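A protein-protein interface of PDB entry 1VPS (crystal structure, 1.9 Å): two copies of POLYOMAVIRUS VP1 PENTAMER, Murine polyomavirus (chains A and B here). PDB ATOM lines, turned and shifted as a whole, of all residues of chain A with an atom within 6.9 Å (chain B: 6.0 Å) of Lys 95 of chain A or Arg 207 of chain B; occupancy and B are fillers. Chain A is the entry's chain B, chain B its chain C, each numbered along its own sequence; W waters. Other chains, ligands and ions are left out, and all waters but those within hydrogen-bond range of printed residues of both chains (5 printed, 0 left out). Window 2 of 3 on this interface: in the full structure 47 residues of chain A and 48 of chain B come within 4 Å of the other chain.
The side-chain carboxylate (OE1) of Glu 97 of chain A sits at hydrogen-bond distance from the side-chain hydroxyl (OH) of Tyr 208 of chain B (2.7 Å).
OG1 of Thr 225 of chain A lies within hydrogen-bond range of O of Tyr 208 of chain B (2.6 Å).
ND2 of Asn 226 of chain A sits at hydrogen-bond distance from O of Asn 203 of chain B, 3.4 Å away.
The side-chain amide nitrogen (ND2) of Asn 226 of chain A lies within hydrogen-bond range of the backbone carbonyl oxygen (O) of Thr 206 of chain B (2.9 Å).
The backbone carbonyl oxygen (O) of Asn 226 of chain A is in hydrogen-bond range of the guanidinium group (NH1) of Arg 207 of chain B (3.4 Å).
OD1 of Asn 226 of chain A is in hydrogen-bond range of N of Tyr 208 of chain B (3.0 Å).
The backbone carbonyl oxygen (O) of Asn 226 of chain A lies within hydrogen-bond range of the side-chain amino group (NZ) of Lys 95 of chain A (2.8 Å).
N of Lys 95 of chain A is in hydrogen-bond range of O of Lys 276 of chain A, at 2.9 Å.
The backbone carbonyl oxygen (O) of Glu 97 of chain A sits at hydrogen-bond distance from the backbone NH (N) of Tyr 274 of chain A, at 2.8 Å.
The side-chain hydroxyl (OG1) of Thr 227 of chain A lies within hydrogen-bond range of the side-chain hydroxyl (OG1) of Thr 225 of chain A, 2.8 Å away.
The backbone NH of Phe 209 of chain B lies within hydrogen-bond range of the backbone carbonyl oxygen of Phe 134 of chain B (2.9 Å).
The backbone carbonyl oxygen (O) of Val 136 of chain B lies within hydrogen-bond range of the backbone NH (N) of Arg 207 of chain B (2.9 Å).
Hydrophobic or aromatic side chains of chain B that line the printed part of chain A: Tyr 208 and Phe 209.
Of the 16 printed residues of chain A, 5 touch a printed residue of chain B.
Water W5 bridges the side-chain amino group (NZ) of Lys 276 of chain A and the side-chain carboxylate (OE1) of Glu 204 of chain B.
Water W3 lies within hydrogen-bond range of OE1 of Glu 235 of chain B, NH2 of Arg 207 of chain B and NZ of Lys 95 of chain A.
Water W4 lies within hydrogen-bond range of the side-chain amide nitrogen of Asn 226 of chain A (3.0 Å) and the backbone carbonyl oxygen of Asn 203 of chain B (3.5 Å).
Water W2 bridges the backbone carbonyl oxygen of Thr 227 of chain A (3.1 Å) and the guanidinium group of Arg 207 of chain B (3.3 Å).
Water W1 lies within hydrogen-bond range of the guanidinium group of Arg 207 of chain B (3.1 Å), the side-chain amino group of Lys 95 of chain A (3.2 Å) and the side-chain carboxylate of Glu 235 of chain B (3.5 Å).
Lys 95 of chain A touches one residue of chain B.
Arg 207 of chain B touches just these residues of chain A: Lys 95 (3.9 Å), Asn 226 (3.4 Å) and Thr 227 (3.6 Å).
Of the printed residues of chain B, Glu 97 of chain A touches Tyr 208 (2.7 Å).
Of the printed residues of chain B, Thr 225 of chain A touches Tyr 208 and Phe 209.
Printed residues of chain A within 4 Å of Thr 206 of chain B: Asn 226 (2.9 Å).
Printed residues of chain B within 4 Å of Asn 226 of chain A: Asn 203, Thr 206, Arg 207 and Tyr 208.
Printed residues of chain A within 4 Å of Phe 209 of chain B: Thr 225 and Thr 227.
Thr 278 of chain A touches none of the printed residues of chain B.
The nearest printed residue of chain A that does not touch Phe 209 of chain B is Asn 226 of chain A (5.5 Å).
No position is printed for both chains.
Among the printed residues, pairs that only touch across the chains: Thr 227 of chain A with Phe 209 of chain B, Thr 227 of chain A with Arg 207 of chain B, Thr 225 of chain A with Phe 209 of chain B and Lys 95 of chain A with Arg 207 of chain B.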
ATOM      1  N   SER A  93     -10.034   0.124   4.587  1.00  0.00           N
ATOM      2  CA  SER A  93     -10.800   0.186   5.821  1.00  0.00           C
ATOM      3  C   SER A  93     -12.109  -0.570   5.674  1.00  0.00           C
ATOM      4  O   SER A  93     -12.485  -0.977   4.569  1.00  0.00           O
ATOM      5  CB  SER A  93     -11.100   1.648   6.158  1.00  0.00           C
ATOM      6  OG  SER A  93     -11.801   2.274   5.093  1.00  0.00           O
ATOM      7  N   VAL A  94     -12.819  -0.710   6.787  1.00  0.00           N
ATOM      8  CA  VAL A  94     -14.091  -1.405   6.797  1.00  0.00           C
ATOM      9  C   VAL A  94     -15.008  -0.832   7.869  1.00  0.00           C
ATOM     10  O   VAL A  94     -14.556  -0.463   8.955  1.00  0.00           O
ATOM     11  CB  VAL A  94     -13.896  -2.941   7.073  1.00  0.00           C
ATOM     12  CG1 VAL A  94     -13.177  -3.173   8.402  1.00  0.00           C
ATOM     13  CG2 VAL A  94     -15.240  -3.677   7.071  1.00  0.00           C
ATOM     14  N   LYS A  95     -16.268  -0.648   7.510  1.00  0.00           N
ATOM     15  CA  LYS A  95     -17.274  -0.207   8.458  1.00  0.00           C
ATOM     16  C   LYS A  95     -18.011  -1.507   8.743  1.00  0.00           C
ATOM     17  O   LYS A  95     -18.562  -2.125   7.826  1.00  0.00           O
ATOM     18  CB  LYS A  95     -18.244   0.791   7.833  1.00  0.00           C
ATOM     19  CG  LYS A  95     -17.772   2.222   7.876  1.00  0.00           C
ATOM     20  CD  LYS A  95     -18.922   3.134   7.554  1.00  0.00           C
ATOM     21  CE  LYS A  95     -18.531   4.559   7.780  1.00  0.00           C
ATOM     22  NZ  LYS A  95     -19.648   5.459   7.387  1.00  0.00           N
ATOM     23  N   THR A  96     -17.955  -1.969   9.981  1.00  0.00           N
ATOM     24  CA  THR A  96     -18.619  -3.211  10.328  1.00  0.00           C
ATOM     25  C   THR A  96     -19.543  -2.986  11.516  1.00  0.00           C
ATOM     26  O   THR A  96     -19.255  -2.162  12.395  1.00  0.00           O
ATOM     27  CB  THR A  96     -17.597  -4.337  10.587  1.00  0.00           C
ATOM     28  OG1 THR A  96     -18.291  -5.569  10.794  1.00  0.00           O
ATOM     29  CG2 THR A  96     -16.718  -4.022  11.794  1.00  0.00           C
ATOM     30  N   GLU A  97     -20.641  -3.733  11.544  1.00  0.00           N
ATOM     31  CA  GLU A  97     -21.639  -3.574  12.587  1.00  0.00           C
ATOM     32  C   GLU A  97     -22.386  -4.874  12.848  1.00  0.00           C
ATOM     33  O   GLU A  97     -22.730  -5.589  11.904  1.00  0.00           O
ATOM     34  CB  GLU A  97     -22.631  -2.504  12.121  1.00  0.00           C
ATOM     35  CG  GLU A  97     -23.719  -2.134  13.109  1.00  0.00           C
ATOM     36  CD  GLU A  97     -24.549  -0.954  12.632  1.00  0.00           C
ATOM     37  OE1 GLU A  97     -23.987  -0.034  12.003  1.00  0.00           O
ATOM     38  OE2 GLU A  97     -25.763  -0.939  12.890  1.00  0.00           O
ATOM     39  N   THR A 225     -23.151   1.737  15.263  1.00  0.00           N
ATOM     40  CA  THR A 225     -23.251   3.063  14.663  1.00  0.00           C
ATOM     41  C   THR A 225     -22.679   2.987  13.257  1.00  0.00           C
ATOM     42  O   THR A 225     -21.774   2.186  12.996  1.00  0.00           O
ATOM     43  CB  THR A 225     -22.439   4.144  15.463  1.00  0.00           C
ATOM     44  OG1 THR A 225     -22.484   5.395  14.765  1.00  0.00           O
ATOM     45  CG2 THR A 225     -20.977   3.733  15.630  1.00  0.00           C
ATOM     46  N   ASN A 226     -23.184   3.825  12.358  1.00  0.00           N
ATOM     47  CA  ASN A 226     -22.670   3.845  10.997  1.00  0.00           C
ATOM     48  C   ASN A 226     -21.607   4.937  10.827  1.00  0.00           C
ATOM     49  O   ASN A 226     -21.260   5.303   9.704  1.00  0.00           O
ATOM     50  CB  ASN A 226     -23.805   4.001   9.968  1.00  0.00           C
ATOM     51  CG  ASN A 226     -24.542   5.336  10.070  1.00  0.00           C
ATOM     52  OD1 ASN A 226     -24.535   5.996  11.110  1.00  0.00           O
ATOM     53  ND2 ASN A 226     -25.229   5.705   8.998  1.00  0.00           N
ATOM     54  N   THR A 227     -21.061   5.425  11.940  1.00  0.00           N
ATOM     55  CA  THR A 227     -20.048   6.478  11.897  1.00  0.00           C
ATOM     56  C   THR A 227     -18.642   5.995  12.260  1.00  0.00           C
ATOM     57  O   THR A 227     -17.699   6.785  12.286  1.00  0.00           O
ATOM     58  CB  THR A 227     -20.406   7.619  12.871  1.00  0.00           C
ATOM     59  OG1 THR A 227     -20.379   7.113  14.213  1.00  0.00           O
ATOM     60  CG2 THR A 227     -21.803   8.165  12.580  1.00  0.00           C
ATOM     61  N   LEU A 228     -18.498   4.707  12.549  1.00  0.00           N
ATOM     62  CA  LEU A 228     -17.204   4.162  12.943  1.00  0.00           C
ATOM     63  C   LEU A 228     -16.518   3.348  11.848  1.00  0.00           C
ATOM     64  O   LEU A 228     -17.051   2.336  11.381  1.00  0.00           O
ATOM     65  CB  LEU A 228     -17.361   3.310  14.212  1.00  0.00           C
ATOM     66  CG  LEU A 228     -16.133   2.639  14.855  1.00  0.00           C
ATOM     67  CD1 LEU A 228     -15.118   3.695  15.309  1.00  0.00           C
ATOM     68  CD2 LEU A 228     -16.571   1.776  16.053  1.00  0.00           C
ATOM     69  N   THR A 229     -15.320   3.788  11.476  1.00  0.00           N
ATOM     70  CA  THR A 229     -14.503   3.140  10.454  1.00  0.00           C
ATOM     71  C   THR A 229     -13.307   2.432  11.096  1.00  0.00           C
ATOM     72  O   THR A 229     -12.645   2.999  11.965  1.00  0.00           O
ATOM     73  CB  THR A 229     -13.966   4.194   9.464  1.00  0.00           C
ATOM     74  OG1 THR A 229     -15.068   4.836   8.809  1.00  0.00           O
ATOM     75  CG2 THR A 229     -13.051   3.563   8.433  1.00  0.00           C
ATOM     76  N   THR A 230     -13.061   1.183  10.707  1.00  0.00           N
ATOM     77  CA  THR A 230     -11.921   0.419  11.222  1.00  0.00           C
ATOM     78  C   THR A 230     -10.830   0.483  10.147  1.00  0.00           C
ATOM     79  O   THR A 230     -11.042   0.049   9.013  1.00  0.00           O
ATOM     80  CB  THR A 230     -12.290  -1.065  11.463  1.00  0.00           C
ATOM     81  OG1 THR A 230     -13.407  -1.141  12.355  1.00  0.00           O
ATOM     82  CG2 THR A 230     -11.115  -1.831  12.060  1.00  0.00           C
ATOM     83  N   TYR A 274     -22.525  -6.969   9.507  1.00  0.00           N
ATOM     84  CA  TYR A 274     -22.443  -6.253   8.242  1.00  0.00           C
ATOM     85  C   TYR A 274     -21.013  -5.777   7.993  1.00  0.00           C
ATOM     86  O   TYR A 274     -20.296  -5.425   8.935  1.00  0.00           O
ATOM     87  CB  TYR A 274     -23.400  -5.060   8.282  1.00  0.00           C
ATOM     88  CG  TYR A 274     -23.212  -4.053   7.176  1.00  0.00           C
ATOM     89  CD1 TYR A 274     -23.843  -4.216   5.942  1.00  0.00           C
ATOM     90  CD2 TYR A 274     -22.405  -2.923   7.371  1.00  0.00           C
ATOM     91  CE1 TYR A 274     -23.684  -3.278   4.927  1.00  0.00           C
ATOM     92  CE2 TYR A 274     -22.238  -1.978   6.363  1.00  0.00           C
ATOM     93  CZ  TYR A 274     -22.880  -2.161   5.140  1.00  0.00           C
ATOM     94  OH  TYR A 274     -22.735  -1.212   4.144  1.00  0.00           O
ATOM     95  N   PHE A 275     -20.609  -5.773   6.724  1.00  0.00           N
ATOM     96  CA  PHE A 275     -19.278  -5.329   6.320  1.00  0.00           C
ATOM     97  C   PHE A 275     -19.398  -4.408   5.111  1.00  0.00           C
ATOM     98  O   PHE A 275     -20.154  -4.699   4.180  1.00  0.00           O
ATOM     99  CB  PHE A 275     -18.403  -6.496   5.836  1.00  0.00           C
ATOM    100  CG  PHE A 275     -18.008  -7.486   6.896  1.00  0.00           C
ATOM    101  CD1 PHE A 275     -18.890  -8.492   7.295  1.00  0.00           C
ATOM    102  CD2 PHE A 275     -16.709  -7.494   7.402  1.00  0.00           C
ATOM    103  CE1 PHE A 275     -18.478  -9.497   8.175  1.00  0.00           C
ATOM    104  CE2 PHE A 275     -16.283  -8.490   8.281  1.00  0.00           C
ATOM    105  CZ  PHE A 275     -17.170  -9.498   8.666  1.00  0.00           C
ATOM    106  N   LYS A 276     -18.663  -3.301   5.131  1.00  0.00           N
ATOM    107  CA  LYS A 276     -18.601  -2.390   3.991  1.00  0.00           C
ATOM    108  C   LYS A 276     -17.114  -2.084   3.862  1.00  0.00           C
ATOM    109  O   LYS A 276     -16.559  -1.323   4.663  1.00  0.00           O
ATOM    110  CB  LYS A 276     -19.410  -1.118   4.220  1.00  0.00           C
ATOM    111  CG  LYS A 276     -19.293  -0.122   3.065  1.00  0.00           C
ATOM    112  CD  LYS A 276     -20.477   0.842   3.019  1.00  0.00           C
ATOM    113  CE  LYS A 276     -20.752   1.480   4.379  1.00  0.00           C
ATOM    114  NZ  LYS A 276     -21.990   2.302   4.328  1.00  0.00           N
ATOM    115  N   ILE A 277     -16.453  -2.771   2.933  1.00  0.00           N
ATOM    116  CA  ILE A 277     -15.018  -2.607   2.725  1.00  0.00           C
ATOM    117  C   ILE A 277     -14.658  -1.620   1.611  1.00  0.00           C
ATOM    118  O   ILE A 277     -15.234  -1.666   0.523  1.00  0.00           O
ATOM    119  CB  ILE A 277     -14.327  -3.966   2.406  1.00  0.00           C
ATOM    120  CG1 ILE A 277     -14.704  -5.027   3.447  1.00  0.00           C
ATOM    121  CG2 ILE A 277     -12.810  -3.809   2.379  1.00  0.00           C
ATOM    122  CD1 ILE A 277     -15.941  -5.812   3.081  1.00  0.00           C
ATOM    123  N   THR A 278     -13.735  -0.709   1.916  1.00  0.00           N
ATOM    124  CA  THR A 278     -13.241   0.269   0.948  1.00  0.00           C
ATOM    125  C   THR A 278     -11.908  -0.268   0.426  1.00  0.00           C
ATOM    126  O   THR A 278     -11.000  -0.576   1.209  1.00  0.00           O
ATOM    127  CB  THR A 278     -13.019   1.657   1.597  1.00  0.00           C
ATOM    128  OG1 THR A 278     -14.285   2.210   1.964  1.00  0.00           O
ATOM    129  CG2 THR A 278     -12.319   2.617   0.631  1.00  0.00           C
ATOM    130  N   PHE B 134     -29.955   7.056  19.023  1.00  0.00           N
ATOM    131  CA  PHE B 134     -30.434   8.327  18.480  1.00  0.00           C
ATOM    132  C   PHE B 134     -29.883   8.492  17.071  1.00  0.00           C
ATOM    133  O   PHE B 134     -28.820   7.950  16.744  1.00  0.00           O
ATOM    134  CB  PHE B 134     -30.118   9.541  19.373  1.00  0.00           C
ATOM    135  CG  PHE B 134     -28.675   9.949  19.386  1.00  0.00           C
ATOM    136  CD1 PHE B 134     -27.787   9.387  20.298  1.00  0.00           C
ATOM    137  CD2 PHE B 134     -28.207  10.920  18.502  1.00  0.00           C
ATOM    138  CE1 PHE B 134     -26.449   9.787  20.336  1.00  0.00           C
ATOM    139  CE2 PHE B 134     -26.869  11.329  18.528  1.00  0.00           C
ATOM    140  CZ  PHE B 134     -25.987  10.760  19.451  1.00  0.00           C
ATOM    141  N   ALA B 135     -30.647   9.181  16.226  1.00  0.00           N
ATOM    142  CA  ALA B 135     -30.263   9.408  14.842  1.00  0.00           C
ATOM    143  C   ALA B 135     -30.743  10.767  14.353  1.00  0.00           C
ATOM    144  O   ALA B 135     -31.748  11.292  14.839  1.00  0.00           O
ATOM    145  CB  ALA B 135     -30.850   8.308  13.949  1.00  0.00           C
ATOM    146  N   VAL B 136     -30.004  11.332  13.403  1.00  0.00           N
ATOM    147  CA  VAL B 136     -30.347  12.607  12.782  1.00  0.00           C
ATOM    148  C   VAL B 136     -30.095  12.384  11.296  1.00  0.00           C
ATOM    149  O   VAL B 136     -29.046  11.839  10.924  1.00  0.00           O
ATOM    150  CB  VAL B 136     -29.439  13.767  13.275  1.00  0.00           C
ATOM    151  CG1 VAL B 136     -29.784  15.057  12.520  1.00  0.00           C
ATOM    152  CG2 VAL B 136     -29.611  13.987  14.776  1.00  0.00           C
ATOM    153  N   GLY B 137     -31.057  12.757  10.454  1.00  0.00           N
ATOM    154  CA  GLY B 137     -30.881  12.574   9.024  1.00  0.00           C
ATOM    155  C   GLY B 137     -31.806  13.381   8.135  1.00  0.00           C
ATOM    156  O   GLY B 137     -32.727  14.044   8.615  1.00  0.00           O
ATOM    157  N   ASN B 203     -29.212   4.165   4.985  1.00  0.00           N
ATOM    158  CA  ASN B 203     -28.934   5.335   5.836  1.00  0.00           C
ATOM    159  C   ASN B 203     -27.730   6.150   5.379  1.00  0.00           C
ATOM    160  O   ASN B 203     -26.905   6.582   6.185  1.00  0.00           O
ATOM    161  CB  ASN B 203     -28.735   4.917   7.295  1.00  0.00           C
ATOM    162  CG  ASN B 203     -30.020   4.509   7.951  1.00  0.00           C
ATOM    163  OD1 ASN B 203     -30.981   5.281   7.994  1.00  0.00           O
ATOM    164  ND2 ASN B 203     -30.068   3.280   8.439  1.00  0.00           N
ATOM    165  N   GLU B 204     -27.649   6.376   4.076  1.00  0.00           N
ATOM    166  CA  GLU B 204     -26.550   7.133   3.498  1.00  0.00           C
ATOM    167  C   GLU B 204     -26.640   8.602   3.901  1.00  0.00           C
ATOM    168  O   GLU B 204     -25.639   9.318   3.896  1.00  0.00           O
ATOM    169  CB  GLU B 204     -26.591   7.016   1.973  1.00  0.00           C
ATOM    170  CG  GLU B 204     -25.231   6.754   1.345  1.00  0.00           C
ATOM    171  CD  GLU B 204     -24.547   5.523   1.945  1.00  0.00           C
ATOM    172  OE1 GLU B 204     -25.095   4.405   1.790  1.00  0.00           O
ATOM    173  OE2 GLU B 204     -23.472   5.678   2.583  1.00  0.00           O
ATOM    174  N   ASN B 205     -27.833   9.026   4.300  1.00  0.00           N
ATOM    175  CA  ASN B 205     -28.073  10.412   4.676  1.00  0.00           C
ATOM    176  C   ASN B 205     -28.514  10.590   6.130  1.00  0.00           C
ATOM    177  O   ASN B 205     -29.178  11.574   6.470  1.00  0.00           O
ATOM    178  CB  ASN B 205     -29.152  10.971   3.765  1.00  0.00           C
ATOM    179  CG  ASN B 205     -28.847  12.355   3.295  1.00  0.00           C
ATOM    180  OD1 ASN B 205     -27.693  12.814   3.329  1.00  0.00           O
ATOM    181  ND2 ASN B 205     -29.878  13.035   2.814  1.00  0.00           N
ATOM    182  N   THR B 206     -28.122   9.651   6.982  1.00  0.00           N
ATOM    183  CA  THR B 206     -28.478   9.679   8.396  1.00  0.00           C
ATOM    184  C   THR B 206     -27.302   9.151   9.194  1.00  0.00           C
ATOM    185  O   THR B 206     -26.554   8.311   8.694  1.00  0.00           O
ATOM    186  CB  THR B 206     -29.708   8.758   8.652  1.00  0.00           C
ATOM    187  OG1 THR B 206     -30.882   9.366   8.100  1.00  0.00           O
ATOM    188  CG2 THR B 206     -29.915   8.482  10.151  1.00  0.00           C
ATOM    189  N   ARG B 207     -27.087   9.701  10.388  1.00  0.00           N
ATOM    190  CA  ARG B 207     -26.023   9.229  11.278  1.00  0.00           C
ATOM    191  C   ARG B 207     -26.773   8.688  12.504  1.00  0.00           C
ATOM    192  O   ARG B 207     -27.669   9.362  13.029  1.00  0.00           O
ATOM    193  CB  ARG B 207     -25.065  10.366  11.696  1.00  0.00           C
ATOM    194  CG  ARG B 207     -24.490  11.211  10.542  1.00  0.00           C
ATOM    195  CD  ARG B 207     -23.772  10.379   9.474  1.00  0.00           C
ATOM    196  NE  ARG B 207     -22.329  10.290   9.692  1.00  0.00           N
ATOM    197  CZ  ARG B 207     -21.529   9.349   9.169  1.00  0.00           C
ATOM    198  NH1 ARG B 207     -22.029   8.388   8.379  1.00  0.00           N
ATOM    199  NH2 ARG B 207     -20.221   9.360   9.440  1.00  0.00           N
ATOM    200  N   TYR B 208     -26.491   7.447  12.893  1.00  0.00           N
ATOM    201  CA  TYR B 208     -27.151   6.856  14.057  1.00  0.00           C
ATOM    202  C   TYR B 208     -26.113   6.292  15.018  1.00  0.00           C
ATOM    203  O   TYR B 208     -25.039   5.849  14.600  1.00  0.00           O
ATOM    204  CB  TYR B 208     -28.190   5.792  13.651  1.00  0.00           C
ATOM    205  CG  TYR B 208     -27.632   4.581  12.932  1.00  0.00           C
ATOM    206  CD1 TYR B 208     -26.978   3.556  13.634  1.00  0.00           C
ATOM    207  CD2 TYR B 208     -27.760   4.454  11.545  1.00  0.00           C
ATOM    208  CE1 TYR B 208     -26.464   2.443  12.967  1.00  0.00           C
ATOM    209  CE2 TYR B 208     -27.250   3.345  10.873  1.00  0.00           C
ATOM    210  CZ  TYR B 208     -26.605   2.349  11.586  1.00  0.00           C
ATOM    211  OH  TYR B 208     -26.097   1.274  10.905  1.00  0.00           O
ATOM    212  N   PHE B 209     -26.427   6.364  16.310  1.00  0.00           N
ATOM    213  CA  PHE B 209     -25.534   5.905  17.374  1.00  0.00           C
ATOM    214  C   PHE B 209     -26.351   5.111  18.395  1.00  0.00           C
ATOM    215  O   PHE B 209     -27.284   5.646  19.014  1.00  0.00           O
ATOM    216  CB  PHE B 209     -24.906   7.112  18.085  1.00  0.00           C
ATOM    217  CG  PHE B 209     -24.353   8.164  17.149  1.00  0.00           C
ATOM    218  CD1 PHE B 209     -25.202   9.070  16.511  1.00  0.00           C
ATOM    219  CD2 PHE B 209     -22.982   8.262  16.927  1.00  0.00           C
ATOM    220  CE1 PHE B 209     -24.690  10.060  15.668  1.00  0.00           C
ATOM    221  CE2 PHE B 209     -22.459   9.248  16.088  1.00  0.00           C
ATOM    222  CZ  PHE B 209     -23.316  10.150  15.456  1.00  0.00           C
ATOM    223  N   VAL B 231     -20.451  15.221  16.522  1.00  0.00           N
ATOM    224  CA  VAL B 231     -20.156  15.580  15.140  1.00  0.00           C
ATOM    225  C   VAL B 231     -20.961  14.700  14.180  1.00  0.00           C
ATOM    226  O   VAL B 231     -21.001  13.481  14.339  1.00  0.00           O
ATOM    227  CB  VAL B 231     -18.638  15.425  14.867  1.00  0.00           C
ATOM    228  CG1 VAL B 231     -18.346  15.455  13.379  1.00  0.00           C
ATOM    229  CG2 VAL B 231     -17.878  16.542  15.576  1.00  0.00           C
ATOM    230  N   LEU B 232     -21.604  15.317  13.192  1.00  0.00           N
ATOM    231  CA  LEU B 232     -22.402  14.576  12.216  1.00  0.00           C
ATOM    232  C   LEU B 232     -21.757  14.521  10.834  1.00  0.00           C
ATOM    233  O   LEU B 232     -22.312  13.930   9.910  1.00  0.00           O
ATOM    234  CB  LEU B 232     -23.801  15.176  12.111  1.00  0.00           C
ATOM    235  CG  LEU B 232     -24.628  15.145  13.398  1.00  0.00           C
ATOM    236  CD1 LEU B 232     -25.951  15.856  13.182  1.00  0.00           C
ATOM    237  CD2 LEU B 232     -24.846  13.700  13.839  1.00  0.00           C
ATOM    238  N   LEU B 233     -20.598  15.160  10.693  1.00  0.00           N
ATOM    239  CA  LEU B 233     -19.861  15.182   9.428  1.00  0.00           C
ATOM    240  C   LEU B 233     -19.187  13.833   9.179  1.00  0.00           C
ATOM    241  O   LEU B 233     -18.636  13.238  10.111  1.00  0.00           O
ATOM    242  CB  LEU B 233     -18.776  16.265   9.465  1.00  0.00           C
ATOM    243  CG  LEU B 233     -19.209  17.697   9.771  1.00  0.00           C
ATOM    244  CD1 LEU B 233     -17.996  18.609   9.706  1.00  0.00           C
ATOM    245  CD2 LEU B 233     -20.280  18.149   8.788  1.00  0.00           C
ATOM    246  N   ASP B 234     -19.228  13.352   7.936  1.00  0.00           N
ATOM    247  CA  ASP B 234     -18.583  12.080   7.593  1.00  0.00           C
ATOM    248  C   ASP B 234     -17.076  12.246   7.392  1.00  0.00           C
ATOM    249  O   ASP B 234     -16.511  13.303   7.701  1.00  0.00           O
ATOM    250  CB  ASP B 234     -19.236  11.412   6.363  1.00  0.00           C
ATOM    251  CG  ASP B 234     -19.183  12.272   5.088  1.00  0.00           C
ATOM    252  OD1 ASP B 234     -18.263  13.105   4.919  1.00  0.00           O
ATOM    253  OD2 ASP B 234     -20.081  12.095   4.233  1.00  0.00           O
ATOM    254  N   GLU B 235     -16.435  11.224   6.831  1.00  0.00           N
ATOM    255  CA  GLU B 235     -14.990  11.259   6.595  1.00  0.00           C
ATOM    256  C   GLU B 235     -14.554  12.347   5.599  1.00  0.00           C
ATOM    257  O   GLU B 235     -13.402  12.775   5.608  1.00  0.00           O
ATOM    258  CB  GLU B 235     -14.458   9.870   6.180  1.00  0.00           C
ATOM    259  CG  GLU B 235     -14.986   9.306   4.849  1.00  0.00           C
ATOM    260  CD  GLU B 235     -16.352   8.604   4.946  1.00  0.00           C
ATOM    261  OE1 GLU B 235     -16.921   8.486   6.062  1.00  0.00           O
ATOM    262  OE2 GLU B 235     -16.856   8.158   3.887  1.00  0.00           O
ATOM    263  N   VAL B 238     -18.629  16.186   5.167  1.00  0.00           N
ATOM    264  CA  VAL B 238     -19.995  16.486   4.749  1.00  0.00           C
ATOM    265  C   VAL B 238     -20.960  15.785   5.700  1.00  0.00           C
ATOM    266  O   VAL B 238     -20.791  14.604   5.989  1.00  0.00           O
ATOM    267  CB  VAL B 238     -20.277  15.990   3.309  1.00  0.00           C
ATOM    268  CG1 VAL B 238     -21.659  16.446   2.860  1.00  0.00           C
ATOM    269  CG2 VAL B 238     -19.202  16.487   2.351  1.00  0.00           C
ATOM    270  N   PRO B 240     -25.191  15.031   7.005  1.00  0.00           N
ATOM    271  CA  PRO B 240     -26.427  14.625   6.328  1.00  0.00           C
ATOM    272  C   PRO B 240     -27.031  15.818   5.587  1.00  0.00           C
ATOM    273  O   PRO B 240     -27.084  16.929   6.123  1.00  0.00           O
ATOM    274  CB  PRO B 240     -27.328  14.213   7.492  1.00  0.00           C
ATOM    275  CG  PRO B 240     -26.371  13.778   8.535  1.00  0.00           C
ATOM    276  CD  PRO B 240     -25.299  14.817   8.457  1.00  0.00           C
HETATM  277  O   HOH W   1     -20.339   8.129   5.747  1.00  0.00           O
HETATM  278  O   HOH W   2     -17.598   9.713  11.353  1.00  0.00           O
HETATM  279  O   HOH W   3     -18.085   7.729   8.506  1.00  0.00           O
HETATM  280  O   HOH W   4     -25.138   3.686   6.849  1.00  0.00           O
HETATM  281  O   HOH W   5     -24.633   1.935   3.713  1.00  0.00           O
